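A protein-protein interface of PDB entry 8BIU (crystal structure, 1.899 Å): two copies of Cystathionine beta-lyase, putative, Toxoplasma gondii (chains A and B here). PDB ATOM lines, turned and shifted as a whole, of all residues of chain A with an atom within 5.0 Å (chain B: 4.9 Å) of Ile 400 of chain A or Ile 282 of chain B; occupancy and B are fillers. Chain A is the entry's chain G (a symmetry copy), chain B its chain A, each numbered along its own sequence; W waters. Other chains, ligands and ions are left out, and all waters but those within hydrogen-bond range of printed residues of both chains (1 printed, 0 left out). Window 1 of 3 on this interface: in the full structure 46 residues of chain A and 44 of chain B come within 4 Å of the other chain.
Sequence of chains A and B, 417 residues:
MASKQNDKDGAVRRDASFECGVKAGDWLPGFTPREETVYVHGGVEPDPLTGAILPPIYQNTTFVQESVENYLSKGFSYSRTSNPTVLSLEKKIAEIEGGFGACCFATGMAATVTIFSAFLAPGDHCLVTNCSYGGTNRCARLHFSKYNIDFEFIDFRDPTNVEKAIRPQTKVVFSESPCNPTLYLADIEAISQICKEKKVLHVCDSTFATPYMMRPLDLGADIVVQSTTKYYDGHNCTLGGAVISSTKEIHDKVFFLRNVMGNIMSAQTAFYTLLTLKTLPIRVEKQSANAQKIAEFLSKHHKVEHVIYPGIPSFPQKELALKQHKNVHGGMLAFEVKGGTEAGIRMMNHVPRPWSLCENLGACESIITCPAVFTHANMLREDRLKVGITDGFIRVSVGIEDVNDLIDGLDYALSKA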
ATOM      1  N   ILE A 282     -18.040  28.841  17.758  1.00  0.00           N
ATOM      2  CA  ILE A 282     -16.795  28.080  17.766  1.00  0.00           C
ATOM      3  C   ILE A 282     -15.772  28.689  16.810  1.00  0.00           C
ATOM      4  O   ILE A 282     -14.562  28.677  17.085  1.00  0.00           O
ATOM      5  CB  ILE A 282     -17.076  26.609  17.428  1.00  0.00           C
ATOM      6  CG1 ILE A 282     -17.806  26.499  16.092  1.00  0.00           C
ATOM      7  CG2 ILE A 282     -17.927  25.976  18.498  1.00  0.00           C
ATOM      8  CD1 ILE A 282     -17.925  25.061  15.591  1.00  0.00           C
ATOM      9  N   ARG A 283     -16.236  29.235  15.686  1.00  0.00           N
ATOM     10  CA  ARG A 283     -15.353  29.975  14.795  1.00  0.00           C
ATOM     11  C   ARG A 283     -14.681  31.120  15.536  1.00  0.00           C
ATOM     12  O   ARG A 283     -13.460  31.290  15.453  1.00  0.00           O
ATOM     13  CB  ARG A 283     -16.134  30.517  13.595  1.00  0.00           C
ATOM     14  CG  ARG A 283     -16.357  29.500  12.501  1.00  0.00           C
ATOM     15  CD  ARG A 283     -16.940  30.123  11.236  1.00  0.00           C
ATOM     16  NE  ARG A 283     -18.359  30.460  11.324  1.00  0.00           N
ATOM     17  CZ  ARG A 283     -18.826  31.702  11.358  1.00  0.00           C
ATOM     18  NH1 ARG A 283     -17.988  32.715  11.331  1.00  0.00           N
ATOM     19  NH2 ARG A 283     -20.126  31.933  11.412  1.00  0.00           N
ATOM     20  N   LYS A 286     -12.151  30.131  18.104  1.00  0.00           N
ATOM     21  CA  LYS A 286     -10.869  29.737  17.525  1.00  0.00           C
ATOM     22  C   LYS A 286     -10.099  30.940  17.010  1.00  0.00           C
ATOM     23  O   LYS A 286      -8.894  31.076  17.263  1.00  0.00           O
ATOM     24  CB  LYS A 286     -11.078  28.721  16.406  1.00  0.00           C
ATOM     25  CG  LYS A 286      -9.769  28.250  15.804  1.00  0.00           C
ATOM     26  CD  LYS A 286      -8.948  27.570  16.878  1.00  0.00           C
ATOM     27  CE  LYS A 286      -7.937  26.589  16.320  1.00  0.00           C
ATOM     28  NZ  LYS A 286      -6.639  27.266  16.067  1.00  0.00           N
ATOM     29  N   GLN A 287     -10.770  31.802  16.258  1.00  0.00           N
ATOM     30  CA  GLN A 287     -10.121  32.988  15.729  1.00  0.00           C
ATOM     31  C   GLN A 287      -9.520  33.825  16.846  1.00  0.00           C
ATOM     32  O   GLN A 287      -8.404  34.319  16.715  1.00  0.00           O
ATOM     33  CB  GLN A 287     -11.120  33.803  14.924  1.00  0.00           C
ATOM     34  CG  GLN A 287     -11.625  33.075  13.712  1.00  0.00           C
ATOM     35  CD  GLN A 287     -12.769  33.791  13.071  1.00  0.00           C
ATOM     36  OE1 GLN A 287     -13.872  33.807  13.606  1.00  0.00           O
ATOM     37  NE2 GLN A 287     -12.512  34.431  11.945  1.00  0.00           N
ATOM     38  N   ASN A 290      -6.386  32.138  18.323  1.00  0.00           N
ATOM     39  CA  ASN A 290      -5.302  32.415  17.385  1.00  0.00           C
ATOM     40  C   ASN A 290      -4.859  33.869  17.465  1.00  0.00           C
ATOM     41  O   ASN A 290      -3.662  34.166  17.386  1.00  0.00           O
ATOM     42  CB  ASN A 290      -5.735  32.086  15.954  1.00  0.00           C
ATOM     43  CG  ASN A 290      -5.712  30.602  15.647  1.00  0.00           C
ATOM     44  OD1 ASN A 290      -5.215  29.790  16.427  1.00  0.00           O
ATOM     45  ND2 ASN A 290      -6.256  30.241  14.492  1.00  0.00           N
ATOM     46  N   ALA A 363     -13.161  35.918   8.383  1.00  0.00           N
ATOM     47  CA  ALA A 363     -13.313  34.642   7.703  1.00  0.00           C
ATOM     48  C   ALA A 363     -12.450  33.564   8.351  1.00  0.00           C
ATOM     49  O   ALA A 363     -11.494  33.853   9.071  1.00  0.00           O
ATOM     50  CB  ALA A 363     -12.950  34.788   6.228  1.00  0.00           C
ATOM     51  N   CYS A 364     -12.805  32.302   8.081  1.00  0.00           N
ATOM     52  CA  CYS A 364     -11.908  31.202   8.424  1.00  0.00           C
ATOM     53  C   CYS A 364     -10.544  31.354   7.769  1.00  0.00           C
ATOM     54  O   CYS A 364      -9.548  30.876   8.323  1.00  0.00           O
ATOM     55  CB  CYS A 364     -12.512  29.842   8.043  1.00  0.00           C
ATOM     56  SG  CYS A 364     -14.217  29.484   8.540  1.00  0.00           S
ATOM     57  N   SER A 366      -7.358  33.413   6.989  1.00  0.00           N
ATOM     58  CA  SER A 366      -6.647  34.560   7.534  1.00  0.00           C
ATOM     59  C   SER A 366      -6.313  35.556   6.427  1.00  0.00           C
ATOM     60  O   SER A 366      -5.836  35.182   5.353  1.00  0.00           O
ATOM     61  CB  SER A 366      -5.379  34.098   8.246  1.00  0.00           C
ATOM     62  OG  SER A 366      -5.711  33.528   9.497  1.00  0.00           O
ATOM     63  N   VAL A 398      -7.695  37.282  11.704  1.00  0.00           N
ATOM     64  CA  VAL A 398      -7.188  35.963  12.047  1.00  0.00           C
ATOM     65  C   VAL A 398      -8.286  34.949  11.777  1.00  0.00           C
ATOM     66  O   VAL A 398      -9.429  35.118  12.229  1.00  0.00           O
ATOM     67  CB  VAL A 398      -6.721  35.914  13.515  1.00  0.00           C
ATOM     68  CG1 VAL A 398      -6.261  34.525  13.881  1.00  0.00           C
ATOM     69  CG2 VAL A 398      -5.607  36.928  13.752  1.00  0.00           C
ATOM     70  N   GLY A 399      -7.948  33.918  11.011  1.00  0.00           N
ATOM     71  CA  GLY A 399      -8.851  32.837  10.717  1.00  0.00           C
ATOM     72  C   GLY A 399      -8.678  31.691  11.686  1.00  0.00           C
ATOM     73  O   GLY A 399      -8.239  31.865  12.827  1.00  0.00           O
ATOM     74  N   ILE A 400      -9.023  30.498  11.229  1.00  0.00           N
ATOM     75  CA  ILE A 400      -8.968  29.339  12.095  1.00  0.00           C
ATOM     76  C   ILE A 400      -7.904  28.350  11.631  1.00  0.00           C
ATOM     77  O   ILE A 400      -7.976  27.173  11.951  1.00  0.00           O
ATOM     78  CB  ILE A 400     -10.347  28.674  12.223  1.00  0.00           C
ATOM     79  CG1 ILE A 400     -10.820  28.141  10.874  1.00  0.00           C
ATOM     80  CG2 ILE A 400     -11.355  29.683  12.755  1.00  0.00           C
ATOM     81  CD1 ILE A 400     -12.167  27.444  10.946  1.00  0.00           C
ATOM     82  N   GLU A 401      -6.906  28.815  10.891  1.00  0.00           N
ATOM     83  CA  GLU A 401      -5.801  27.941  10.545  1.00  0.00           C
ATOM     84  C   GLU A 401      -4.976  27.640  11.790  1.00  0.00           C
ATOM     85  O   GLU A 401      -5.157  28.237  12.851  1.00  0.00           O
ATOM     86  CB  GLU A 401      -4.914  28.573   9.467  1.00  0.00           C
ATOM     87  CG  GLU A 401      -5.603  28.914   8.148  1.00  0.00           C
ATOM     88  CD  GLU A 401      -6.059  30.350   8.095  1.00  0.00           C
ATOM     89  OE1 GLU A 401      -6.347  30.910   9.167  1.00  0.00           O
ATOM     90  OE2 GLU A 401      -6.119  30.923   6.985  1.00  0.00           O
ATOM     91  N   ASP A 402      -4.046  26.705  11.648  1.00  0.00           N
ATOM     92  CA  ASP A 402      -3.089  26.456  12.713  1.00  0.00           C
ATOM     93  C   ASP A 402      -2.274  27.718  12.942  1.00  0.00           C
ATOM     94  O   ASP A 402      -1.720  28.284  11.996  1.00  0.00           O
ATOM     95  CB  ASP A 402      -2.182  25.285  12.357  1.00  0.00           C
ATOM     96  CG  ASP A 402      -1.335  24.844  13.522  1.00  0.00           C
ATOM     97  OD1 ASP A 402      -0.368  25.555  13.867  1.00  0.00           O
ATOM     98  OD2 ASP A 402      -1.654  23.796  14.111  1.00  0.00           O
ATOM     99  N   GLU B  36      -5.141  21.807  10.622  1.00  0.00           N
ATOM    100  CA  GLU B  36      -6.260  22.737  10.485  1.00  0.00           C
ATOM    101  C   GLU B  36      -6.083  23.650   9.286  1.00  0.00           C
ATOM    102  O   GLU B  36      -7.066  24.010   8.622  1.00  0.00           O
ATOM    103  CB  GLU B  36      -6.425  23.575  11.751  1.00  0.00           C
ATOM    104  CG  GLU B  36      -6.403  22.800  13.053  1.00  0.00           C
ATOM    105  CD  GLU B  36      -6.396  23.720  14.257  1.00  0.00           C
ATOM    106  OE1 GLU B  36      -5.293  24.139  14.673  1.00  0.00           O
ATOM    107  OE2 GLU B  36      -7.498  24.043  14.768  1.00  0.00           O
ATOM    108  N   VAL B  40      -8.637  24.292   6.096  1.00  0.00           N
ATOM    109  CA  VAL B  40      -9.098  25.592   5.617  1.00  0.00           C
ATOM    110  C   VAL B  40      -8.768  25.782   4.139  1.00  0.00           C
ATOM    111  O   VAL B  40      -9.597  26.275   3.363  1.00  0.00           O
ATOM    112  CB  VAL B  40      -8.511  26.726   6.468  1.00  0.00           C
ATOM    113  CG1 VAL B  40      -8.867  28.063   5.848  1.00  0.00           C
ATOM    114  CG2 VAL B  40      -9.039  26.647   7.885  1.00  0.00           C
ATOM    115  N   LYS B 278     -13.984  23.329   6.082  1.00  0.00           N
ATOM    116  CA  LYS B 278     -13.093  24.255   6.761  1.00  0.00           C
ATOM    117  C   LYS B 278     -13.276  24.210   8.268  1.00  0.00           C
ATOM    118  O   LYS B 278     -12.320  24.443   9.010  1.00  0.00           O
ATOM    119  CB  LYS B 278     -13.331  25.684   6.287  1.00  0.00           C
ATOM    120  CG  LYS B 278     -13.131  25.974   4.813  1.00  0.00           C
ATOM    121  CD  LYS B 278     -13.921  27.238   4.540  1.00  0.00           C
ATOM    122  CE  LYS B 278     -13.517  27.963   3.282  1.00  0.00           C
ATOM    123  NZ  LYS B 278     -14.344  29.207   3.146  1.00  0.00           N
ATOM    124  N   THR B 279     -14.490  23.954   8.740  1.00  0.00           N
ATOM    125  CA  THR B 279     -14.759  23.946  10.167  1.00  0.00           C
ATOM    126  C   THR B 279     -14.868  22.547  10.746  1.00  0.00           C
ATOM    127  O   THR B 279     -15.264  22.415  11.903  1.00  0.00           O
ATOM    128  CB  THR B 279     -16.042  24.729  10.484  1.00  0.00           C
ATOM    129  OG1 THR B 279     -17.162  24.110   9.843  1.00  0.00           O
ATOM    130  CG2 THR B 279     -15.921  26.164  10.002  1.00  0.00           C
ATOM    131  N   LEU B 280     -14.519  21.506   9.995  1.00  0.00           N
ATOM    132  CA  LEU B 280     -14.639  20.160  10.545  1.00  0.00           C
ATOM    133  C   LEU B 280     -13.867  19.982  11.850  1.00  0.00           C
ATOM    134  O   LEU B 280     -14.423  19.401  12.790  1.00  0.00           O
ATOM    135  CB  LEU B 280     -14.208  19.123   9.504  1.00  0.00           C
ATOM    136  CG  LEU B 280     -14.541  17.726  10.028  1.00  0.00           C
ATOM    137  CD1 LEU B 280     -14.858  16.764   8.913  1.00  0.00           C
ATOM    138  CD2 LEU B 280     -13.407  17.176  10.907  1.00  0.00           C
ATOM    139  N   PRO B 281     -12.610  20.419  11.974  1.00  0.00           N
ATOM    140  CA  PRO B 281     -11.905  20.206  13.253  1.00  0.00           C
ATOM    141  C   PRO B 281     -12.597  20.846  14.446  1.00  0.00           C
ATOM    142  O   PRO B 281     -12.788  20.184  15.474  1.00  0.00           O
ATOM    143  CB  PRO B 281     -10.524  20.818  12.985  1.00  0.00           C
ATOM    144  CG  PRO B 281     -10.326  20.641  11.528  1.00  0.00           C
ATOM    145  CD  PRO B 281     -11.688  20.817  10.899  1.00  0.00           C
ATOM    146  N   ILE B 282     -12.990  22.117  14.343  1.00  0.00           N
ATOM    147  CA  ILE B 282     -13.615  22.776  15.488  1.00  0.00           C
ATOM    148  C   ILE B 282     -15.000  22.203  15.755  1.00  0.00           C
ATOM    149  O   ILE B 282     -15.401  22.040  16.917  1.00  0.00           O
ATOM    150  CB  ILE B 282     -13.657  24.301  15.281  1.00  0.00           C
ATOM    151  CG1 ILE B 282     -14.522  24.680  14.082  1.00  0.00           C
ATOM    152  CG2 ILE B 282     -12.260  24.837  15.102  1.00  0.00           C
ATOM    153  CD1 ILE B 282     -14.601  26.186  13.843  1.00  0.00           C
ATOM    154  N   ARG B 283     -15.746  21.875  14.693  1.00  0.00           N
ATOM    155  CA  ARG B 283     -17.036  21.225  14.874  1.00  0.00           C
ATOM    156  C   ARG B 283     -16.883  19.924  15.634  1.00  0.00           C
ATOM    157  O   ARG B 283     -17.633  19.660  16.578  1.00  0.00           O
ATOM    158  CB  ARG B 283     -17.715  20.940  13.534  1.00  0.00           C
ATOM    159  CG  ARG B 283     -18.215  22.159  12.786  1.00  0.00           C
ATOM    160  CD  ARG B 283     -19.093  21.756  11.604  1.00  0.00           C
ATOM    161  NE  ARG B 283     -18.321  21.433  10.406  1.00  0.00           N
ATOM    162  CZ  ARG B 283     -18.268  20.225   9.854  1.00  0.00           C
ATOM    163  NH1 ARG B 283     -18.936  19.223  10.397  1.00  0.00           N
ATOM    164  NH2 ARG B 283     -17.544  20.018   8.764  1.00  0.00           N
ATOM    165  N   VAL B 284     -15.962  19.071  15.192  1.00  0.00           N
ATOM    166  CA  VAL B 284     -15.849  17.749  15.787  1.00  0.00           C
ATOM    167  C   VAL B 284     -15.319  17.851  17.212  1.00  0.00           C
ATOM    168  O   VAL B 284     -15.727  17.088  18.096  1.00  0.00           O
ATOM    169  CB  VAL B 284     -14.980  16.842  14.902  1.00  0.00           C
ATOM    170  CG1 VAL B 284     -14.635  15.558  15.618  1.00  0.00           C
ATOM    171  CG2 VAL B 284     -15.720  16.523  13.615  1.00  0.00           C
ATOM    172  N   GLU B 285     -14.438  18.818  17.478  1.00  0.00           N
ATOM    173  CA  GLU B 285     -14.028  19.039  18.859  1.00  0.00           C
ATOM    174  C   GLU B 285     -15.229  19.383  19.736  1.00  0.00           C
ATOM    175  O   GLU B 285     -15.407  18.791  20.810  1.00  0.00           O
ATOM    176  CB  GLU B 285     -12.960  20.132  18.932  1.00  0.00           C
ATOM    177  CG  GLU B 285     -11.582  19.697  18.402  1.00  0.00           C
ATOM    178  CD  GLU B 285     -10.727  18.940  19.429  1.00  0.00           C
ATOM    179  OE1 GLU B 285      -9.638  18.460  19.055  1.00  0.00           O
ATOM    180  OE2 GLU B 285     -11.130  18.825  20.604  1.00  0.00           O
ATOM    181  N   LYS B 286     -16.070  20.334  19.300  1.00  0.00           N
ATOM    182  CA  LYS B 286     -17.219  20.723  20.120  1.00  0.00           C
ATOM    183  C   LYS B 286     -18.210  19.571  20.274  1.00  0.00           C
ATOM    184  O   LYS B 286     -18.679  19.279  21.381  1.00  0.00           O
ATOM    185  CB  LYS B 286     -17.909  21.940  19.521  1.00  0.00           C
ATOM    186  CG  LYS B 286     -19.097  22.436  20.329  1.00  0.00           C
ATOM    187  CD  LYS B 286     -18.681  22.763  21.752  1.00  0.00           C
ATOM    188  CE  LYS B 286     -19.697  23.660  22.446  1.00  0.00           C
ATOM    189  NZ  LYS B 286     -20.863  22.896  22.941  1.00  0.00           N
HETATM  190  O   HOH W   1      -3.440  21.852  13.294  1.00  0.00           O
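Ile 282 of chain B touches its own counterpart, Ile 282 of chain A.
Ile 282 of chain A touches Arg 283 of chain B, and with the chains exchanged Arg 283 of chain A touches Ile 282 of chain B.
3 positions are printed for both chains.
Of the 10 pairs that touch across the chains among the printed residues, 3 have their exchanged pair printed and touching as well.
The side-chain amino group (NZ) of Lys 286 of chain A lies within salt-bridge range of the side-chain carboxylate (OE2) of Glu 36 of chain B (3.6 Å).
Ile 282 of chain A touches Ile 282 of chain B.
CD1 of Ile 282 of chain A touches N of Arg 283 of chain B (3.96 Å).
Arg 283 of chain A touches Ile 282 of chain B (N to CD1, 3.9 Å).
Val 40 of chain B touches Cys 364 of chain A.
O of Ile 400 of chain A touches CB of Glu 36 of chain B, 3.9 Å away.
Ile 400 of chain A touches Val 40 of chain B.
O of Lys 278 of chain B touches CD1 of Ile 400 of chain A, at 3.6 Å.
Ile 400 of chain A touches Ile 282 of chain B (CD1 to CD1, 3.99 Å).
Asp 402 of chain A touches Glu 36 of chain B (OD2 to OE1, 3.7 Å).
OG1 of Thr 279 of chain B lies within hydrogen-bond range of NE of Arg 283 of chain B (3.0 Å).
The backbone carbonyl oxygen of Arg 283 of chain A lies close to the side-chain amide oxygen of Gln 287 of chain A (3.1 Å).
The side-chain amino group (NZ) of Lys 286 of chain A is in hydrogen-bond range of the side-chain amide oxygen (OD1) of Asn 290 of chain A (2.9 Å).
The backbone carbonyl oxygen (O) of Cys 364 of chain A lies within hydrogen-bond range of the backbone NH (N) of Ile 400 of chain A, 3.0 Å away.
Water W1 bridges the side-chain carboxylate of Asp 402 of chain A (2.8 Å) and the backbone NH of Glu 36 of chain B (3.2 Å).
Of the printed residues of chain B, Ile 282 of chain A touches Ile 282 (3.7 Å) and Arg 283 (3.96 Å).
Of the printed residues of chain B, Arg 283 of chain A touches Ile 282.
Of the printed residues of chain B, Lys 286 of chain A touches Glu 36.
Printed residues of chain B within 4 Å of Ile 400 of chain A: Glu 36 (3.9 Å), Val 40 (3.8 Å), Lys 278 (3.6 Å) and Ile 282 (3.99 Å).
Of the printed residues of chain A, Ile 282 of chain B touches Ile 282 (3.7 Å), Arg 283 (3.9 Å) and Ile 400 (3.99 Å).
The nearest printed residue of chain A that does not touch Ile 282 of chain B is Lys 286 of chain A (4.3 Å).
Of the 13 printed residues of chain A, 6 touch a printed residue of chain B.
Along chain B the printed residues that touch a printed residue of chain A span positions 36 to 283.
Among the printed residues, 10 pairs touch across the chains.
Among the printed residues, Asp or Glu carboxylates within 4 Å of a Lys or Arg side-chain nitrogen of the other chain: Lys 286 of chain A with Glu 36 of chain B (3.6 Å).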
